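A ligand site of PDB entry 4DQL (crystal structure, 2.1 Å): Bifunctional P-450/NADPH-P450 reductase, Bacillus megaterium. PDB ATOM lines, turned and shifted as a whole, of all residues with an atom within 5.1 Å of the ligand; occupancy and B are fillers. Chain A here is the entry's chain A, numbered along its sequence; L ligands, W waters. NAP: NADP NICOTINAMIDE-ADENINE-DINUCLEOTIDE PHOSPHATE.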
ATOM      1  N   GLN A  18      25.899  20.427 -39.284  1.00  0.00           N
ATOM      2  CA  GLN A  18      26.825  19.393 -39.006  1.00  0.00           C
ATOM      3  C   GLN A  18      28.092  19.559 -39.888  1.00  0.00           C
ATOM      4  O   GLN A  18      28.090  20.373 -40.795  1.00  0.00           O
ATOM      5  CB  GLN A  18      26.205  18.023 -39.174  1.00  0.00           C
ATOM      6  CG  GLN A  18      25.023  17.778 -38.224  1.00  0.00           C
ATOM      7  CD  GLN A  18      24.734  16.312 -37.999  1.00  0.00           C
ATOM      8  OE1 GLN A  18      25.644  15.452 -38.038  1.00  0.00           O
ATOM      9  NE2 GLN A  18      23.443  16.018 -37.654  1.00  0.00           N
ATOM     10  N   ARG A  24      25.039  12.537 -41.204  1.00  0.00           N
ATOM     11  CA  ARG A  24      23.733  13.095 -40.860  1.00  0.00           C
ATOM     12  C   ARG A  24      23.663  14.535 -41.109  1.00  0.00           C
ATOM     13  O   ARG A  24      24.679  15.182 -41.257  1.00  0.00           O
ATOM     14  CB  ARG A  24      23.356  12.798 -39.419  1.00  0.00           C
ATOM     15  CG  ARG A  24      23.278  11.282 -39.194  1.00  0.00           C
ATOM     16  CD  ARG A  24      22.627  10.933 -37.905  1.00  0.00           C
ATOM     17  NE  ARG A  24      23.338  11.629 -36.845  1.00  0.00           N
ATOM     18  CZ  ARG A  24      22.836  11.932 -35.654  1.00  0.00           C
ATOM     19  NH1 ARG A  24      21.592  11.537 -35.348  1.00  0.00           N
ATOM     20  NH2 ARG A  24      23.581  12.624 -34.781  1.00  0.00           N
ATOM     21  N   THR A  26      21.581  18.312 -40.048  1.00  0.00           N
ATOM     22  CA  THR A  26      20.714  19.112 -39.188  1.00  0.00           C
ATOM     23  C   THR A  26      20.794  20.446 -39.807  1.00  0.00           C
ATOM     24  O   THR A  26      21.863  20.907 -39.964  1.00  0.00           O
ATOM     25  CB  THR A  26      21.299  19.220 -37.730  1.00  0.00           C
ATOM     26  OG1 THR A  26      21.496  17.917 -37.220  1.00  0.00           O
ATOM     27  CG2 THR A  26      20.365  19.982 -36.859  1.00  0.00           C
ATOM     28  N   SER A 192      16.450  18.440 -37.535  1.00  0.00           N
ATOM     29  CA  SER A 192      17.101  17.228 -37.781  1.00  0.00           C
ATOM     30  C   SER A 192      16.439  16.513 -39.042  1.00  0.00           C
ATOM     31  O   SER A 192      15.211  16.319 -39.126  1.00  0.00           O
ATOM     32  CB  SER A 192      16.982  16.373 -36.544  1.00  0.00           C
ATOM     33  OG  SER A 192      17.521  15.147 -36.907  1.00  0.00           O
ATOM     34  N   VAL A 193      17.271  16.155 -40.017  1.00  0.00           N
ATOM     35  CA  VAL A 193      16.793  15.561 -41.238  1.00  0.00           C
ATOM     36  C   VAL A 193      16.616  14.090 -41.079  1.00  0.00           C
ATOM     37  O   VAL A 193      17.553  13.382 -40.894  1.00  0.00           O
ATOM     38  CB  VAL A 193      17.709  15.864 -42.392  1.00  0.00           C
ATOM     39  CG1 VAL A 193      17.204  15.184 -43.769  1.00  0.00           C
ATOM     40  CG2 VAL A 193      17.790  17.380 -42.568  1.00  0.00           C
ATOM     41  N   VAL A 194      15.372  13.638 -41.117  1.00  0.00           N
ATOM     42  CA  VAL A 194      15.073  12.253 -40.905  1.00  0.00           C
ATOM     43  C   VAL A 194      15.295  11.490 -42.217  1.00  0.00           C
ATOM     44  O   VAL A 194      14.776  11.850 -43.258  1.00  0.00           O
ATOM     45  CB  VAL A 194      13.661  12.026 -40.379  1.00  0.00           C
ATOM     46  CG1 VAL A 194      13.324  10.552 -40.301  1.00  0.00           C
ATOM     47  CG2 VAL A 194      13.493  12.677 -38.988  1.00  0.00           C
ATOM     48  N   PRO A 248      20.250  17.583 -25.460  1.00  0.00           N
ATOM     49  CA  PRO A 248      21.201  17.011 -26.405  1.00  0.00           C
ATOM     50  C   PRO A 248      20.706  16.972 -27.839  1.00  0.00           C
ATOM     51  O   PRO A 248      19.462  17.031 -28.090  1.00  0.00           O
ATOM     52  CB  PRO A 248      21.471  15.639 -25.851  1.00  0.00           C
ATOM     53  CG  PRO A 248      20.255  15.328 -25.012  1.00  0.00           C
ATOM     54  CD  PRO A 248      19.771  16.619 -24.499  1.00  0.00           C
ATOM     55  N   GLY A 249      21.630  17.081 -28.789  1.00  0.00           N
ATOM     56  CA  GLY A 249      21.295  17.061 -30.228  1.00  0.00           C
ATOM     57  C   GLY A 249      20.411  18.228 -30.540  1.00  0.00           C
ATOM     58  O   GLY A 249      20.636  19.368 -30.083  1.00  0.00           O
ATOM     59  N   THR A 250      19.345  17.968 -31.296  1.00  0.00           N
ATOM     60  CA  THR A 250      18.419  18.970 -31.713  1.00  0.00           C
ATOM     61  C   THR A 250      17.642  19.540 -30.536  1.00  0.00           C
ATOM     62  O   THR A 250      16.983  20.540 -30.675  1.00  0.00           O
ATOM     63  CB  THR A 250      17.468  18.267 -32.790  1.00  0.00           C
ATOM     64  OG1 THR A 250      18.277  18.068 -33.967  1.00  0.00           O
ATOM     65  CG2 THR A 250      16.394  19.071 -33.162  1.00  0.00           C
ATOM     66  N   GLY A 251      17.632  18.850 -29.405  1.00  0.00           N
ATOM     67  CA  GLY A 251      17.091  19.460 -28.162  1.00  0.00           C
ATOM     68  C   GLY A 251      17.726  20.768 -27.725  1.00  0.00           C
ATOM     69  O   GLY A 251      17.131  21.493 -26.939  1.00  0.00           O
ATOM     70  N   GLY A 280      24.619  17.335 -25.434  1.00  0.00           N
ATOM     71  CA  GLY A 280      25.219  16.059 -25.781  1.00  0.00           C
ATOM     72  C   GLY A 280      25.129  15.858 -27.298  1.00  0.00           C
ATOM     73  O   GLY A 280      24.170  16.283 -27.923  1.00  0.00           O
ATOM     74  N   CYS A 281      26.173  15.295 -27.866  1.00  0.00           N
ATOM     75  CA  CYS A 281      26.244  14.868 -29.294  1.00  0.00           C
ATOM     76  C   CYS A 281      27.309  13.773 -29.482  1.00  0.00           C
ATOM     77  O   CYS A 281      27.895  13.293 -28.481  1.00  0.00           O
ATOM     78  CB  CYS A 281      26.474  16.059 -30.173  1.00  0.00           C
ATOM     79  SG  CYS A 281      28.185  16.742 -29.941  1.00  0.00           S
ATOM     80  N   ARG A 282      27.464  13.258 -30.694  1.00  0.00           N
ATOM     81  CA  ARG A 282      28.399  12.169 -30.973  1.00  0.00           C
ATOM     82  C   ARG A 282      29.848  12.617 -30.813  1.00  0.00           C
ATOM     83  O   ARG A 282      30.606  11.949 -30.127  1.00  0.00           O
ATOM     84  CB  ARG A 282      28.217  11.652 -32.404  1.00  0.00           C
ATOM     85  CG  ARG A 282      26.908  10.940 -32.649  1.00  0.00           C
ATOM     86  CD  ARG A 282      26.797  10.589 -34.174  1.00  0.00           C
ATOM     87  NE  ARG A 282      25.566   9.852 -34.376  1.00  0.00           N
ATOM     88  CZ  ARG A 282      25.195   9.187 -35.493  1.00  0.00           C
ATOM     89  NH1 ARG A 282      25.980   9.127 -36.577  1.00  0.00           N
ATOM     90  NH2 ARG A 282      23.993   8.555 -35.498  1.00  0.00           N
ATOM     91  N   ASP A 287      28.822  16.709 -34.970  1.00  0.00           N
ATOM     92  CA  ASP A 287      27.459  17.238 -34.744  1.00  0.00           C
ATOM     93  C   ASP A 287      27.297  18.102 -33.472  1.00  0.00           C
ATOM     94  O   ASP A 287      26.217  18.126 -32.834  1.00  0.00           O
ATOM     95  CB  ASP A 287      26.480  16.058 -34.730  1.00  0.00           C
ATOM     96  CG  ASP A 287      26.840  15.053 -33.693  1.00  0.00           C
ATOM     97  OD1 ASP A 287      26.012  14.175 -33.405  1.00  0.00           O
ATOM     98  OD2 ASP A 287      27.944  15.131 -33.080  1.00  0.00           O
ATOM     99  N   ALA A 308      28.603  16.355 -23.364  1.00  0.00           N
ATOM    100  CA  ALA A 308      28.696  14.927 -23.265  1.00  0.00           C
ATOM    101  C   ALA A 308      28.890  14.335 -24.705  1.00  0.00           C
ATOM    102  O   ALA A 308      28.018  14.542 -25.563  1.00  0.00           O
ATOM    103  CB  ALA A 308      27.475  14.376 -22.656  1.00  0.00           C
ATOM    104  N   SER A 310      29.245  11.115 -27.104  1.00  0.00           N
ATOM    105  CA  SER A 310      28.915   9.730 -27.053  1.00  0.00           C
ATOM    106  C   SER A 310      29.770   8.769 -27.922  1.00  0.00           C
ATOM    107  O   SER A 310      29.746   7.554 -27.686  1.00  0.00           O
ATOM    108  CB  SER A 310      27.406   9.553 -27.401  1.00  0.00           C
ATOM    109  OG  SER A 310      27.104  10.082 -28.668  1.00  0.00           O
ATOM    110  N   ARG A 311      30.538   9.281 -28.867  1.00  0.00           N
ATOM    111  CA  ARG A 311      31.232   8.407 -29.839  1.00  0.00           C
ATOM    112  C   ARG A 311      32.630   8.955 -30.168  1.00  0.00           C
ATOM    113  O   ARG A 311      32.967   9.223 -31.323  1.00  0.00           O
ATOM    114  CB  ARG A 311      30.372   8.336 -31.135  1.00  0.00           C
ATOM    115  CG  ARG A 311      28.976   7.726 -30.916  1.00  0.00           C
ATOM    116  CD  ARG A 311      28.295   7.429 -32.276  1.00  0.00           C
ATOM    117  NE  ARG A 311      26.866   7.177 -32.089  1.00  0.00           N
ATOM    118  CZ  ARG A 311      26.041   6.708 -33.009  1.00  0.00           C
ATOM    119  NH1 ARG A 311      26.538   6.351 -34.219  1.00  0.00           N
ATOM    120  NH2 ARG A 311      24.745   6.530 -32.698  1.00  0.00           N
ATOM    121  N   LYS A 317      31.554   6.307 -23.798  1.00  0.00           N
ATOM    122  CA  LYS A 317      30.305   6.892 -24.255  1.00  0.00           C
ATOM    123  C   LYS A 317      29.703   7.717 -23.105  1.00  0.00           C
ATOM    124  O   LYS A 317      29.484   7.173 -22.054  1.00  0.00           O
ATOM    125  CB  LYS A 317      29.345   5.776 -24.636  1.00  0.00           C
ATOM    126  CG  LYS A 317      28.091   6.296 -25.378  1.00  0.00           C
ATOM    127  CD  LYS A 317      26.847   5.520 -25.033  1.00  0.00           C
ATOM    128  CE  LYS A 317      26.487   4.374 -25.922  1.00  0.00           C
ATOM    129  NZ  LYS A 317      25.301   3.633 -25.230  1.00  0.00           N
ATOM    130  N   TYR A 319      26.670  10.386 -21.931  1.00  0.00           N
ATOM    131  CA  TYR A 319      25.411  11.086 -22.159  1.00  0.00           C
ATOM    132  C   TYR A 319      25.216  12.252 -21.135  1.00  0.00           C
ATOM    133  O   TYR A 319      25.843  12.237 -20.076  1.00  0.00           O
ATOM    134  CB  TYR A 319      24.284  10.097 -21.951  1.00  0.00           C
ATOM    135  CG  TYR A 319      24.115   9.015 -23.070  1.00  0.00           C
ATOM    136  CD1 TYR A 319      24.616   9.217 -24.393  1.00  0.00           C
ATOM    137  CD2 TYR A 319      23.332   7.865 -22.830  1.00  0.00           C
ATOM    138  CE1 TYR A 319      24.393   8.215 -25.418  1.00  0.00           C
ATOM    139  CE2 TYR A 319      23.103   6.896 -23.831  1.00  0.00           C
ATOM    140  CZ  TYR A 319      23.642   7.064 -25.120  1.00  0.00           C
ATOM    141  OH  TYR A 319      23.381   6.103 -26.118  1.00  0.00           O
ATOM    142  N   VAL A 320      24.321  13.178 -21.438  1.00  0.00           N
ATOM    143  CA  VAL A 320      24.035  14.251 -20.540  1.00  0.00           C
ATOM    144  C   VAL A 320      23.772  13.789 -19.105  1.00  0.00           C
ATOM    145  O   VAL A 320      24.306  14.397 -18.160  1.00  0.00           O
ATOM    146  CB  VAL A 320      22.956  15.187 -21.032  1.00  0.00           C
ATOM    147  CG1 VAL A 320      23.490  15.902 -22.215  1.00  0.00           C
ATOM    148  CG2 VAL A 320      21.606  14.456 -21.306  1.00  0.00           C
ATOM    149  N   GLN A 321      22.968  12.753 -18.927  1.00  0.00           N
ATOM    150  CA  GLN A 321      22.667  12.328 -17.567  1.00  0.00           C
ATOM    151  C   GLN A 321      23.875  11.791 -16.801  1.00  0.00           C
ATOM    152  O   GLN A 321      23.850  11.727 -15.561  1.00  0.00           O
ATOM    153  CB  GLN A 321      21.531  11.291 -17.534  1.00  0.00           C
ATOM    154  CG  GLN A 321      21.826  10.012 -18.352  1.00  0.00           C
ATOM    155  CD  GLN A 321      21.260  10.091 -19.794  1.00  0.00           C
ATOM    156  OE1 GLN A 321      21.246  11.134 -20.417  1.00  0.00           O
ATOM    157  NE2 GLN A 321      20.884   8.947 -20.337  1.00  0.00           N
ATOM    158  N   GLN A 349      13.498   8.213 -24.908  1.00  0.00           N
ATOM    159  CA  GLN A 349      14.516   7.572 -24.047  1.00  0.00           C
ATOM    160  C   GLN A 349      15.315   8.630 -23.238  1.00  0.00           C
ATOM    161  O   GLN A 349      15.547   8.456 -22.070  1.00  0.00           O
ATOM    162  CB  GLN A 349      15.538   6.713 -24.841  1.00  0.00           C
ATOM    163  CG  GLN A 349      15.014   5.577 -25.803  1.00  0.00           C
ATOM    164  CD  GLN A 349      14.088   4.421 -25.174  1.00  0.00           C
ATOM    165  OE1 GLN A 349      14.452   3.752 -24.181  1.00  0.00           O
ATOM    166  NE2 GLN A 349      12.929   4.164 -25.849  1.00  0.00           N
ATOM    167  N   MET A 350      15.789   9.657 -23.868  1.00  0.00           N
ATOM    168  CA  MET A 350      16.628  10.641 -23.159  1.00  0.00           C
ATOM    169  C   MET A 350      15.846  11.297 -21.987  1.00  0.00           C
ATOM    170  O   MET A 350      16.252  11.207 -20.856  1.00  0.00           O
ATOM    171  CB  MET A 350      17.118  11.736 -24.107  1.00  0.00           C
ATOM    172  CG  MET A 350      18.128  12.742 -23.425  1.00  0.00           C
ATOM    173  SD  MET A 350      17.212  14.131 -22.738  1.00  0.00           S
ATOM    174  CE  MET A 350      16.479  14.999 -24.131  1.00  0.00           C
ATOM    175  N   ALA A 353      15.266   9.299 -18.902  1.00  0.00           N
ATOM    176  CA  ALA A 353      16.460   8.920 -18.175  1.00  0.00           C
ATOM    177  C   ALA A 353      17.017  10.160 -17.406  1.00  0.00           C
ATOM    178  O   ALA A 353      17.552   9.996 -16.378  1.00  0.00           O
ATOM    179  CB  ALA A 353      17.533   8.241 -19.124  1.00  0.00           C
ATOM    180  N   GLY A 393      10.702  10.228 -31.776  1.00  0.00           N
ATOM    181  CA  GLY A 393      11.541  10.280 -32.993  1.00  0.00           C
ATOM    182  C   GLY A 393      11.697   8.993 -33.811  1.00  0.00           C
ATOM    183  O   GLY A 393      11.984   9.085 -35.021  1.00  0.00           O
HETATM  184  PA  NAP L   1      20.753  12.251 -31.625  1.00  0.00           P
HETATM  185  O1A NAP L   1      21.693  12.955 -32.443  1.00  0.00           O
HETATM  186  O2A NAP L   1      20.181  11.004 -32.044  1.00  0.00           O
HETATM  187  O5B NAP L   1      21.414  12.103 -30.140  1.00  0.00           O
HETATM  188  C5B NAP L   1      21.922  13.294 -29.535  1.00  0.00           C
HETATM  189  C4B NAP L   1      22.924  12.807 -28.527  1.00  0.00           C
HETATM  190  O4B NAP L   1      22.100  12.157 -27.551  1.00  0.00           O
HETATM  191  C3B NAP L   1      23.919  11.768 -29.103  1.00  0.00           C
HETATM  192  O3B NAP L   1      25.173  11.812 -28.461  1.00  0.00           O
HETATM  193  C2B NAP L   1      23.267  10.472 -28.761  1.00  0.00           C
HETATM  194  O2B NAP L   1      24.185   9.443 -28.520  1.00  0.00           O
HETATM  195  C1B NAP L   1      22.585  10.884 -27.376  1.00  0.00           C
HETATM  196  N9A NAP L   1      21.646   9.889 -26.827  1.00  0.00           N
HETATM  197  C8A NAP L   1      21.111   8.722 -27.468  1.00  0.00           C
HETATM  198  N7A NAP L   1      20.367   8.045 -26.527  1.00  0.00           N
HETATM  199  C5A NAP L   1      20.381   8.753 -25.381  1.00  0.00           C
HETATM  200  C6A NAP L   1      19.779   8.545 -24.136  1.00  0.00           C
HETATM  201  N6A NAP L   1      19.053   7.422 -23.880  1.00  0.00           N
HETATM  202  N1A NAP L   1      20.123   9.377 -23.105  1.00  0.00           N
HETATM  203  C2A NAP L   1      20.856  10.487 -23.344  1.00  0.00           C
HETATM  204  N3A NAP L   1      21.361  10.736 -24.565  1.00  0.00           N
HETATM  205  C4A NAP L   1      21.191   9.874 -25.544  1.00  0.00           C
HETATM  206  O3  NAP L   1      19.765  13.476 -31.659  1.00  0.00           O
HETATM  207  PN  NAP L   1      19.358  14.321 -32.955  1.00  0.00           P
HETATM  208  O1N NAP L   1      18.848  15.625 -32.575  1.00  0.00           O
HETATM  209  O2N NAP L   1      20.378  14.315 -34.018  1.00  0.00           O
HETATM  210  O5D NAP L   1      18.072  13.436 -33.559  1.00  0.00           O
HETATM  211  C5D NAP L   1      18.166  12.460 -34.599  1.00  0.00           C
HETATM  212  C4D NAP L   1      17.011  11.390 -34.654  1.00  0.00           C
HETATM  213  O4D NAP L   1      16.567  10.938 -33.385  1.00  0.00           O
HETATM  214  C3D NAP L   1      15.719  11.805 -35.444  1.00  0.00           C
HETATM  215  O3D NAP L   1      16.001  12.840 -36.362  1.00  0.00           O
HETATM  216  C2D NAP L   1      15.134  10.612 -36.273  1.00  0.00           C
HETATM  217  P2B NAP L   1      24.255   7.962 -29.348  1.00  0.00           P
HETATM  218  O1X NAP L   1      25.726   7.843 -29.631  1.00  0.00           O
HETATM  219  O2X NAP L   1      23.555   8.267 -30.623  1.00  0.00           O
HETATM  220  O3X NAP L   1      24.074   6.827 -28.412  1.00  0.00           O
HETATM  221  O   HOH W   1      18.433  12.658 -38.222  1.00  0.00           O
HETATM  222  O   HOH W   2      19.110  12.236 -27.245  1.00  0.00           O
HETATM  223  O   HOH W   3      17.833  10.903 -30.366  1.00  0.00           O
HETATM  224  O   HOH W   4      23.771  14.435 -32.132  1.00  0.00           O
HETATM  225  O   HOH W   5      21.378  17.100 -34.672  1.00  0.00           O
HETATM  226  O   HOH W   6      23.437   9.880 -32.579  1.00  0.00           O
HETATM  227  O   HOH W   7      17.214  14.732 -30.349  1.00  0.00           O
HETATM  228  O   HOH W   8      18.202   5.145 -25.754  1.00  0.00           O
HETATM  229  O   HOH W   9      25.493  12.448 -25.680  1.00  0.00           O
HETATM  230  O   HOH W  10      13.204  14.272 -35.849  1.00  0.00           O
HETATM  231  O   HOH W  11      27.349   5.464 -28.531  1.00  0.00           O
HETATM  232  O   HOH W  12      23.316  12.906 -24.165  1.00  0.00           O
HETATM  233  O   HOH W  13      17.777   9.982 -27.748  1.00  0.00           O
HETATM  234  O   HOH W  14      18.593   5.823 -21.603  1.00  0.00           O
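O3B of the ligand lies close to O of Cys 281 (3.1 Å).
OG of Ser 310 lies within hydrogen-bond range of O3B of the ligand, at 2.6 Å.
An oxygen (O3X) of the ligand is in hydrogen-bond range of the side-chain hydroxyl (OH) of Tyr 319 (2.5 Å).
An oxygen (O3D) of the ligand lies within hydrogen-bond range of the side-chain hydroxyl (OG) of Ser 192.
N1A of the ligand is in hydrogen-bond range of NE2 of Gln 321 (2.9 Å).
The backbone NH (N) of Thr 250 lies within hydrogen-bond range of an oxygen (O1N) of the ligand (2.7 Å).
O1X of the ligand lies within salt-bridge range of NE of Arg 311, at 2.8 Å.
The guanidinium group (NH2) of Arg 24 lies within salt-bridge range of an oxygen (O1A) of the ligand, 3.0 Å away.
The side-chain hydroxyl of Thr 250 lies within hydrogen-bond range of an oxygen (O1N) of the ligand (2.9 Å).
O of Arg 282 lies within hydrogen-bond range of N of Ser 310 (3.4 Å).
The side-chain carboxylate of Asp 287 sits close to the side-chain sulfur of Cys 281, 3.5 Å away.
The backbone carbonyl oxygen (O) of Arg 24 lies close to the side-chain amide oxygen (OE1) of Gln 18 (3.4 Å).
O of Ala 308 is in hydrogen-bond range of N of Cys 281 (3.0 Å).
The backbone carbonyl oxygen (O) of Cys 281 sits at hydrogen-bond distance from the backbone NH (N) of Ser 310.
The side-chain carboxylate (OD1) of Asp 287 is in salt-bridge range of the guanidinium group (NH2) of Arg 24, 3.2 Å away.
OD2 of Asp 287 lies within hydrogen-bond range of N of Arg 282, at 3.1 Å.
The backbone carbonyl oxygen of Gly 280 lies within hydrogen-bond range of the backbone NH of Gly 249.
Val 194 touches the ligand.
Pro 248 touches the ligand.
Gly 249 touches the ligand.
Gly 280 touches the ligand (O to C4B, 3.7 Å).
Arg 282 touches the ligand.
CB of Gln 349 touches N6A of the ligand, at 3.7 Å.
CG of Met 350 touches C2A of the ligand, 3.5 Å away.
Gly 393 touches the ligand (O to C2D, 3.7 Å).
Hydrophobic or aromatic side chains that line the ligand: Val 194, Pro 248, Tyr 319 and Met 350.
Within 4 Å of the ligand: Arg 24, Ser 192, Val 194, Pro 248, Gly 249, Thr 250, Gly 280, Cys 281, Arg 282, Ser 310, Arg 311, Tyr 319, Gln 321, Gln 349, Met 350 and Gly 393.
The nearest printed residue that does not touch the ligand is Lys 317 (4.2 Å).
Water W6 lies within hydrogen-bond range of O2X of the ligand and NE of Arg 282.
Water W4 lies within hydrogen-bond range of O1A of the ligand (2.6 Å), OD1 of Asp 287 (2.6 Å) and NH2 of Arg 24 (3.2 Å).
Water W9 bridges O3B of the ligand and O of Ala 308.
Water W12 bridges the backbone NH of Val 320 (2.9 Å) and a nitrogen (N3A) of the ligand (2.9 Å).
Water W5 lies within hydrogen-bond range of the side-chain hydroxyl of Thr 26, an oxygen (O2N) of the ligand and the side-chain hydroxyl of Thr 250.
Water W1 lies within hydrogen-bond range of O of Val 193, OG of Ser 192 and O3D of the ligand.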
